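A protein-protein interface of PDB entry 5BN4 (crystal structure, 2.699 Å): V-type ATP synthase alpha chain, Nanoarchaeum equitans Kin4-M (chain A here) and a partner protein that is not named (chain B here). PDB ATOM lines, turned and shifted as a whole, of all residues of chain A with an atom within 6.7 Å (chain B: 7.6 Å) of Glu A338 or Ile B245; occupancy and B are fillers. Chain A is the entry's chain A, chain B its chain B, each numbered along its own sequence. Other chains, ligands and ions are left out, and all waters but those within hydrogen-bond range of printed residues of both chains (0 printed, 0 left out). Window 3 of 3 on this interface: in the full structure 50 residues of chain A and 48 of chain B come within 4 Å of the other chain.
Among the printed residues, pairs that only touch across the chains: Glu A331 with Ala B253, Glu A338 with Ile B245, Pro A340 with Ile B245 and Arg A335 with Tyr B254.
Hydrophobic or aromatic side chains of chain A within 4 Å of the printed part of chain B: Pro A340. Of the 13 printed residues of chain B, 4 touch a printed residue of chain A. Printed residues of chain B that touch a printed residue of chain A: Glu B244, Ile B245, Ala B253 and Tyr B254. Hydrophobic or aromatic side chains of chain B that line the printed part of chain A: Ile B245, Ala B253 and Tyr B254. Among the printed residues, 6 pairs touch across the chains. Among the printed residues, Asp or Glu carboxylates within 4 Å of a Lys or Arg side-chain nitrogen of the other chain: Arg A335 with Glu B244.
Of the printed residues of chain B, Arg A335 touches Glu B244 (3.4 Å) and Tyr B254 (3.6 Å). No residue of chain B comes within 4 Å of Gly A337. Printed residues of chain B within 4 Å of Pro A340: Ile B245 (3.6 Å). Gly A344 touches none of the printed residues of chain B. Ile B245 touches two residues of chain A. Ser B247 touches none of the printed residues of chain A. The nearest residue of chain A that does not touch Ile B245 is Ser A334 (4.4 Å). The nearest printed residue of chain A that does not touch Glu B244 is Glu A331 (6.0 Å).
OE2 of Glu A331 sits close to N of Tyr B254 (3.3 Å). OE1 of Glu B244 lies within salt-bridge range of NH1 of Arg A335 (3.4 Å).
The side-chain carboxylate (OE1) of Glu A331 is in salt-bridge range of the guanidinium group (NE) of Arg A335 (2.9 Å). OE1 of Glu A338 lies within hydrogen-bond range of OG of Ser A333. OE1 of Glu A338 is in hydrogen-bond range of OH of Tyr A348 (2.7 Å). OG of Ser B239 sits at hydrogen-bond distance from OE2 of Glu B244, at 2.9 Å. OE1 of Glu B244 is in salt-bridge range of NH1 of Arg B242 (3.3 Å). OE2 of Glu B244 lies within hydrogen-bond range of OH of Tyr B254, at 2.8 Å.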
ATOM      1  N   LEU A 329      18.438 -19.726 -18.586  1.00  0.00           N
ATOM      2  CA  LEU A 329      18.365 -18.299 -18.886  1.00  0.00           C
ATOM      3  C   LEU A 329      18.069 -18.074 -20.360  1.00  0.00           C
ATOM      4  O   LEU A 329      17.266 -17.212 -20.720  1.00  0.00           O
ATOM      5  CB  LEU A 329      19.677 -17.606 -18.520  1.00  0.00           C
ATOM      6  CG  LEU A 329      19.951 -17.378 -17.035  1.00  0.00           C
ATOM      7  CD1 LEU A 329      21.325 -16.759 -16.848  1.00  0.00           C
ATOM      8  CD2 LEU A 329      18.873 -16.492 -16.432  1.00  0.00           C
ATOM      9  N   GLU A 331      16.497 -20.057 -22.308  1.00  0.00           N
ATOM     10  CA  GLU A 331      15.113 -20.443 -22.563  1.00  0.00           C
ATOM     11  C   GLU A 331      14.117 -19.362 -22.158  1.00  0.00           C
ATOM     12  O   GLU A 331      13.198 -19.049 -22.912  1.00  0.00           O
ATOM     13  CB  GLU A 331      14.776 -21.765 -21.871  1.00  0.00           C
ATOM     14  CG  GLU A 331      14.866 -22.961 -22.797  1.00  0.00           C
ATOM     15  CD  GLU A 331      14.011 -22.788 -24.038  1.00  0.00           C
ATOM     16  OE1 GLU A 331      12.807 -22.483 -23.895  1.00  0.00           O
ATOM     17  OE2 GLU A 331      14.545 -22.942 -25.158  1.00  0.00           O
ATOM     18  N   ILE A 332      14.302 -18.800 -20.969  1.00  0.00           N
ATOM     19  CA  ILE A 332      13.446 -17.719 -20.496  1.00  0.00           C
ATOM     20  C   ILE A 332      13.509 -16.533 -21.453  1.00  0.00           C
ATOM     21  O   ILE A 332      12.481 -15.961 -21.816  1.00  0.00           O
ATOM     22  CB  ILE A 332      13.856 -17.250 -19.087  1.00  0.00           C
ATOM     23  CG1 ILE A 332      13.837 -18.422 -18.103  1.00  0.00           C
ATOM     24  CG2 ILE A 332      12.944 -16.134 -18.611  1.00  0.00           C
ATOM     25  CD1 ILE A 332      12.493 -19.109 -17.997  1.00  0.00           C
ATOM     26  N   SER A 333      14.725 -16.184 -21.864  1.00  0.00           N
ATOM     27  CA  SER A 333      14.957 -15.069 -22.778  1.00  0.00           C
ATOM     28  C   SER A 333      14.208 -15.257 -24.096  1.00  0.00           C
ATOM     29  O   SER A 333      13.675 -14.300 -24.657  1.00  0.00           O
ATOM     30  CB  SER A 333      16.456 -14.907 -23.044  1.00  0.00           C
ATOM     31  OG  SER A 333      16.717 -13.767 -23.843  1.00  0.00           O
ATOM     32  N   SER A 334      14.170 -16.494 -24.579  1.00  0.00           N
ATOM     33  CA  SER A 334      13.472 -16.812 -25.820  1.00  0.00           C
ATOM     34  C   SER A 334      11.983 -16.517 -25.696  1.00  0.00           C
ATOM     35  O   SER A 334      11.437 -15.713 -26.451  1.00  0.00           O
ATOM     36  CB  SER A 334      13.678 -18.281 -26.194  1.00  0.00           C
ATOM     37  OG  SER A 334      15.049 -18.572 -26.392  1.00  0.00           O
ATOM     38  N   ARG A 335      11.339 -17.168 -24.731  1.00  0.00           N
ATOM     39  CA  ARG A 335       9.901 -17.033 -24.524  1.00  0.00           C
ATOM     40  C   ARG A 335       9.499 -15.583 -24.239  1.00  0.00           C
ATOM     41  O   ARG A 335       8.379 -15.172 -24.540  1.00  0.00           O
ATOM     42  CB  ARG A 335       9.443 -17.936 -23.373  1.00  0.00           C
ATOM     43  CG  ARG A 335      10.124 -19.301 -23.318  1.00  0.00           C
ATOM     44  CD  ARG A 335       9.361 -20.373 -24.079  1.00  0.00           C
ATOM     45  NE  ARG A 335       9.968 -21.693 -23.911  1.00  0.00           N
ATOM     46  CZ  ARG A 335       9.422 -22.831 -24.330  1.00  0.00           C
ATOM     47  NH1 ARG A 335       8.247 -22.819 -24.944  1.00  0.00           N
ATOM     48  NH2 ARG A 335      10.049 -23.983 -24.134  1.00  0.00           N
ATOM     49  N   LEU A 336      10.418 -14.812 -23.665  1.00  0.00           N
ATOM     50  CA  LEU A 336      10.156 -13.409 -23.347  1.00  0.00           C
ATOM     51  C   LEU A 336      10.146 -12.518 -24.587  1.00  0.00           C
ATOM     52  O   LEU A 336       9.783 -11.345 -24.513  1.00  0.00           O
ATOM     53  CB  LEU A 336      11.183 -12.878 -22.342  1.00  0.00           C
ATOM     54  CG  LEU A 336      11.018 -13.283 -20.877  1.00  0.00           C
ATOM     55  CD1 LEU A 336      12.163 -12.730 -20.041  1.00  0.00           C
ATOM     56  CD2 LEU A 336       9.683 -12.802 -20.340  1.00  0.00           C
ATOM     57  N   GLY A 337      10.550 -13.075 -25.724  1.00  0.00           N
ATOM     58  CA  GLY A 337      10.606 -12.313 -26.959  1.00  0.00           C
ATOM     59  C   GLY A 337      11.802 -11.382 -26.993  1.00  0.00           C
ATOM     60  O   GLY A 337      11.751 -10.302 -27.583  1.00  0.00           O
ATOM     61  N   GLU A 338      12.884 -11.802 -26.346  1.00  0.00           N
ATOM     62  CA  GLU A 338      14.116 -11.028 -26.341  1.00  0.00           C
ATOM     63  C   GLU A 338      14.984 -11.407 -27.529  1.00  0.00           C
ATOM     64  O   GLU A 338      14.942 -12.543 -28.003  1.00  0.00           O
ATOM     65  CB  GLU A 338      14.889 -11.243 -25.037  1.00  0.00           C
ATOM     66  CG  GLU A 338      14.225 -10.638 -23.811  1.00  0.00           C
ATOM     67  CD  GLU A 338      15.039 -10.833 -22.545  1.00  0.00           C
ATOM     68  OE1 GLU A 338      15.843 -11.788 -22.491  1.00  0.00           O
ATOM     69  OE2 GLU A 338      14.874 -10.029 -21.604  1.00  0.00           O
ATOM     70  N   ILE A 339      15.763 -10.446 -28.012  1.00  0.00           N
ATOM     71  CA  ILE A 339      16.696 -10.693 -29.100  1.00  0.00           C
ATOM     72  C   ILE A 339      17.898 -11.469 -28.579  1.00  0.00           C
ATOM     73  O   ILE A 339      18.541 -11.054 -27.617  1.00  0.00           O
ATOM     74  CB  ILE A 339      17.184  -9.381 -29.738  1.00  0.00           C
ATOM     75  CG1 ILE A 339      15.999  -8.565 -30.254  1.00  0.00           C
ATOM     76  CG2 ILE A 339      18.170  -9.667 -30.861  1.00  0.00           C
ATOM     77  CD1 ILE A 339      16.391  -7.230 -30.845  1.00  0.00           C
ATOM     78  N   PRO A 340      18.195 -12.611 -29.212  1.00  0.00           N
ATOM     79  CA  PRO A 340      19.327 -13.455 -28.822  1.00  0.00           C
ATOM     80  C   PRO A 340      20.657 -12.752 -29.059  1.00  0.00           C
ATOM     81  O   PRO A 340      20.766 -11.904 -29.945  1.00  0.00           O
ATOM     82  CB  PRO A 340      19.212 -14.656 -29.768  1.00  0.00           C
ATOM     83  CG  PRO A 340      17.803 -14.639 -30.249  1.00  0.00           C
ATOM     84  CD  PRO A 340      17.421 -13.201 -30.316  1.00  0.00           C
ATOM     85  N   GLY A 344      22.727 -17.699 -29.175  1.00  0.00           N
ATOM     86  CA  GLY A 344      21.376 -17.816 -28.660  1.00  0.00           C
ATOM     87  C   GLY A 344      21.195 -17.282 -27.254  1.00  0.00           C
ATOM     88  O   GLY A 344      20.082 -16.931 -26.857  1.00  0.00           O
ATOM     89  N   PRO A 346      21.156 -14.883 -23.981  1.00  0.00           N
ATOM     90  CA  PRO A 346      20.820 -13.467 -23.808  1.00  0.00           C
ATOM     91  C   PRO A 346      22.083 -12.625 -23.691  1.00  0.00           C
ATOM     92  O   PRO A 346      23.124 -13.139 -23.280  1.00  0.00           O
ATOM     93  CB  PRO A 346      20.042 -13.447 -22.487  1.00  0.00           C
ATOM     94  CG  PRO A 346      20.450 -14.698 -21.778  1.00  0.00           C
ATOM     95  CD  PRO A 346      20.667 -15.707 -22.861  1.00  0.00           C
ATOM     96  N   ALA A 347      21.993 -11.349 -24.050  1.00  0.00           N
ATOM     97  CA  ALA A 347      23.153 -10.467 -24.023  1.00  0.00           C
ATOM     98  C   ALA A 347      23.620 -10.172 -22.600  1.00  0.00           C
ATOM     99  O   ALA A 347      24.729  -9.679 -22.394  1.00  0.00           O
ATOM    100  CB  ALA A 347      22.857  -9.176 -24.771  1.00  0.00           C
ATOM    101  N   TYR A 348      22.772 -10.476 -21.621  1.00  0.00           N
ATOM    102  CA  TYR A 348      23.107 -10.234 -20.222  1.00  0.00           C
ATOM    103  C   TYR A 348      23.614 -11.487 -19.511  1.00  0.00           C
ATOM    104  O   TYR A 348      23.538 -11.584 -18.288  1.00  0.00           O
ATOM    105  CB  TYR A 348      21.911  -9.649 -19.468  1.00  0.00           C
ATOM    106  CG  TYR A 348      20.616 -10.409 -19.658  1.00  0.00           C
ATOM    107  CD1 TYR A 348      20.371 -11.592 -18.969  1.00  0.00           C
ATOM    108  CD2 TYR A 348      19.630  -9.935 -20.513  1.00  0.00           C
ATOM    109  CE1 TYR A 348      19.186 -12.284 -19.139  1.00  0.00           C
ATOM    110  CE2 TYR A 348      18.442 -10.619 -20.685  1.00  0.00           C
ATOM    111  CZ  TYR A 348      18.226 -11.792 -19.997  1.00  0.00           C
ATOM    112  OH  TYR A 348      17.045 -12.478 -20.167  1.00  0.00           O
ATOM    113  N   SER B 239       9.028 -27.402 -32.957  1.00  0.00           N
ATOM    114  CA  SER B 239       9.653 -26.181 -32.461  1.00  0.00           C
ATOM    115  C   SER B 239       9.560 -25.056 -33.485  1.00  0.00           C
ATOM    116  O   SER B 239       9.445 -23.883 -33.127  1.00  0.00           O
ATOM    117  CB  SER B 239      11.120 -26.444 -32.117  1.00  0.00           C
ATOM    118  OG  SER B 239      11.824 -25.230 -31.924  1.00  0.00           O
ATOM    119  N   ARG B 242       5.991 -23.057 -34.121  1.00  0.00           N
ATOM    120  CA  ARG B 242       5.685 -21.940 -33.236  1.00  0.00           C
ATOM    121  C   ARG B 242       6.533 -20.721 -33.589  1.00  0.00           C
ATOM    122  O   ARG B 242       7.203 -20.695 -34.621  1.00  0.00           O
ATOM    123  CB  ARG B 242       5.920 -22.328 -31.777  1.00  0.00           C
ATOM    124  CG  ARG B 242       6.420 -23.748 -31.597  1.00  0.00           C
ATOM    125  CD  ARG B 242       5.340 -24.643 -31.022  1.00  0.00           C
ATOM    126  NE  ARG B 242       5.203 -24.465 -29.580  1.00  0.00           N
ATOM    127  CZ  ARG B 242       5.833 -25.206 -28.674  1.00  0.00           C
ATOM    128  NH1 ARG B 242       6.646 -26.179 -29.062  1.00  0.00           N
ATOM    129  NH2 ARG B 242       5.650 -24.977 -27.380  1.00  0.00           N
ATOM    130  N   LYS B 243       6.503 -19.715 -32.723  1.00  0.00           N
ATOM    131  CA  LYS B 243       7.288 -18.506 -32.932  1.00  0.00           C
ATOM    132  C   LYS B 243       8.699 -18.704 -32.394  1.00  0.00           C
ATOM    133  O   LYS B 243       9.526 -17.792 -32.442  1.00  0.00           O
ATOM    134  CB  LYS B 243       6.627 -17.311 -32.236  1.00  0.00           C
ATOM    135  CG  LYS B 243       6.927 -17.202 -30.740  1.00  0.00           C
ATOM    136  CD  LYS B 243       5.679 -17.383 -29.882  1.00  0.00           C
ATOM    137  CE  LYS B 243       5.238 -18.838 -29.827  1.00  0.00           C
ATOM    138  NZ  LYS B 243       4.061 -19.031 -28.933  1.00  0.00           N
ATOM    139  N   GLU B 244       8.961 -19.908 -31.894  1.00  0.00           N
ATOM    140  CA  GLU B 244      10.193 -20.215 -31.167  1.00  0.00           C
ATOM    141  C   GLU B 244      11.474 -19.824 -31.897  1.00  0.00           C
ATOM    142  O   GLU B 244      11.687 -20.189 -33.055  1.00  0.00           O
ATOM    143  CB  GLU B 244      10.238 -21.696 -30.778  1.00  0.00           C
ATOM    144  CG  GLU B 244       9.221 -22.087 -29.717  1.00  0.00           C
ATOM    145  CD  GLU B 244       9.492 -23.455 -29.122  1.00  0.00           C
ATOM    146  OE1 GLU B 244       8.772 -23.851 -28.182  1.00  0.00           O
ATOM    147  OE2 GLU B 244      10.429 -24.133 -29.594  1.00  0.00           O
ATOM    148  N   ILE B 245      12.318 -19.066 -31.201  1.00  0.00           N
ATOM    149  CA  ILE B 245      13.621 -18.683 -31.719  1.00  0.00           C
ATOM    150  C   ILE B 245      14.543 -19.895 -31.719  1.00  0.00           C
ATOM    151  O   ILE B 245      14.756 -20.516 -30.676  1.00  0.00           O
ATOM    152  CB  ILE B 245      14.258 -17.566 -30.875  1.00  0.00           C
ATOM    153  CG1 ILE B 245      13.351 -16.335 -30.847  1.00  0.00           C
ATOM    154  CG2 ILE B 245      15.630 -17.210 -31.419  1.00  0.00           C
ATOM    155  CD1 ILE B 245      13.901 -15.192 -30.020  1.00  0.00           C
ATOM    156  N   PRO B 246      15.094 -20.235 -32.892  1.00  0.00           N
ATOM    157  CA  PRO B 246      15.887 -21.455 -33.055  1.00  0.00           C
ATOM    158  C   PRO B 246      17.324 -21.303 -32.568  1.00  0.00           C
ATOM    159  O   PRO B 246      17.877 -20.203 -32.585  1.00  0.00           O
ATOM    160  CB  PRO B 246      15.879 -21.659 -34.570  1.00  0.00           C
ATOM    161  CG  PRO B 246      15.825 -20.270 -35.118  1.00  0.00           C
ATOM    162  CD  PRO B 246      14.982 -19.473 -34.150  1.00  0.00           C
ATOM    163  N   SER B 247      17.915 -22.410 -32.131  1.00  0.00           N
ATOM    164  CA  SER B 247      19.339 -22.445 -31.835  1.00  0.00           C
ATOM    165  C   SER B 247      20.080 -22.790 -33.123  1.00  0.00           C
ATOM    166  O   SER B 247      19.642 -22.423 -34.214  1.00  0.00           O
ATOM    167  CB  SER B 247      19.639 -23.475 -30.741  1.00  0.00           C
ATOM    168  OG  SER B 247      21.001 -23.439 -30.350  1.00  0.00           O
ATOM    169  N   ARG B 248      21.196 -23.499 -33.004  1.00  0.00           N
ATOM    170  CA  ARG B 248      21.950 -23.911 -34.182  1.00  0.00           C
ATOM    171  C   ARG B 248      21.229 -25.006 -34.959  1.00  0.00           C
ATOM    172  O   ARG B 248      20.613 -25.894 -34.370  1.00  0.00           O
ATOM    173  CB  ARG B 248      23.360 -24.366 -33.797  1.00  0.00           C
ATOM    174  CG  ARG B 248      24.360 -23.227 -33.713  1.00  0.00           C
ATOM    175  CD  ARG B 248      24.338 -22.410 -34.995  1.00  0.00           C
ATOM    176  NE  ARG B 248      24.584 -23.237 -36.173  1.00  0.00           N
ATOM    177  CZ  ARG B 248      24.145 -22.950 -37.395  1.00  0.00           C
ATOM    178  NH1 ARG B 248      23.427 -21.855 -37.605  1.00  0.00           N
ATOM    179  NH2 ARG B 248      24.418 -23.762 -38.408  1.00  0.00           N
ATOM    180  N   GLY B 250      18.571 -25.021 -36.464  1.00  0.00           N
ATOM    181  CA  GLY B 250      17.124 -24.986 -36.336  1.00  0.00           C
ATOM    182  C   GLY B 250      16.598 -25.693 -35.100  1.00  0.00           C
ATOM    183  O   GLY B 250      15.427 -25.545 -34.746  1.00  0.00           O
ATOM    184  N   TYR B 251      17.461 -26.467 -34.449  1.00  0.00           N
ATOM    185  CA  TYR B 251      17.074 -27.215 -33.258  1.00  0.00           C
ATOM    186  C   TYR B 251      16.651 -26.281 -32.132  1.00  0.00           C
ATOM    187  O   TYR B 251      17.246 -25.222 -31.946  1.00  0.00           O
ATOM    188  CB  TYR B 251      18.219 -28.112 -32.787  1.00  0.00           C
ATOM    189  CG  TYR B 251      18.524 -29.264 -33.714  1.00  0.00           C
ATOM    190  CD1 TYR B 251      17.656 -30.344 -33.818  1.00  0.00           C
ATOM    191  CD2 TYR B 251      19.681 -29.277 -34.480  1.00  0.00           C
ATOM    192  CE1 TYR B 251      17.933 -31.403 -34.663  1.00  0.00           C
ATOM    193  CE2 TYR B 251      19.966 -30.333 -35.328  1.00  0.00           C
ATOM    194  CZ  TYR B 251      19.089 -31.392 -35.415  1.00  0.00           C
ATOM    195  OH  TYR B 251      19.367 -32.445 -36.256  1.00  0.00           O
ATOM    196  N   PRO B 252      15.610 -26.674 -31.383  1.00  0.00           N
ATOM    197  CA  PRO B 252      15.138 -25.878 -30.247  1.00  0.00           C
ATOM    198  C   PRO B 252      16.218 -25.737 -29.184  1.00  0.00           C
ATOM    199  O   PRO B 252      17.006 -26.661 -28.972  1.00  0.00           O
ATOM    200  CB  PRO B 252      13.961 -26.701 -29.707  1.00  0.00           C
ATOM    201  CG  PRO B 252      14.179 -28.079 -30.223  1.00  0.00           C
ATOM    202  CD  PRO B 252      14.819 -27.902 -31.561  1.00  0.00           C
ATOM    203  N   ALA B 253      16.246 -24.585 -28.524  1.00  0.00           N
ATOM    204  CA  ALA B 253      17.270 -24.289 -27.530  1.00  0.00           C
ATOM    205  C   ALA B 253      17.148 -25.166 -26.284  1.00  0.00           C
ATOM    206  O   ALA B 253      18.087 -25.268 -25.493  1.00  0.00           O
ATOM    207  CB  ALA B 253      17.214 -22.821 -27.152  1.00  0.00           C
ATOM    208  N   TYR B 254      15.990 -25.796 -26.116  1.00  0.00           N
ATOM    209  CA  TYR B 254      15.734 -26.651 -24.963  1.00  0.00           C
ATOM    210  C   TYR B 254      15.905 -28.129 -25.296  1.00  0.00           C
ATOM    211  O   TYR B 254      15.302 -28.985 -24.650  1.00  0.00           O
ATOM    212  CB  TYR B 254      14.322 -26.412 -24.425  1.00  0.00           C
ATOM    213  CG  TYR B 254      13.237 -26.489 -25.479  1.00  0.00           C
ATOM    214  CD1 TYR B 254      12.667 -27.708 -25.835  1.00  0.00           C
ATOM    215  CD2 TYR B 254      12.781 -25.342 -26.117  1.00  0.00           C
ATOM    216  CE1 TYR B 254      11.675 -27.780 -26.801  1.00  0.00           C
ATOM    217  CE2 TYR B 254      11.791 -25.404 -27.080  1.00  0.00           C
ATOM    218  CZ  TYR B 254      11.242 -26.623 -27.418  1.00  0.00           C
ATOM    219  OH  TYR B 254      10.257 -26.684 -28.378  1.00  0.00           O
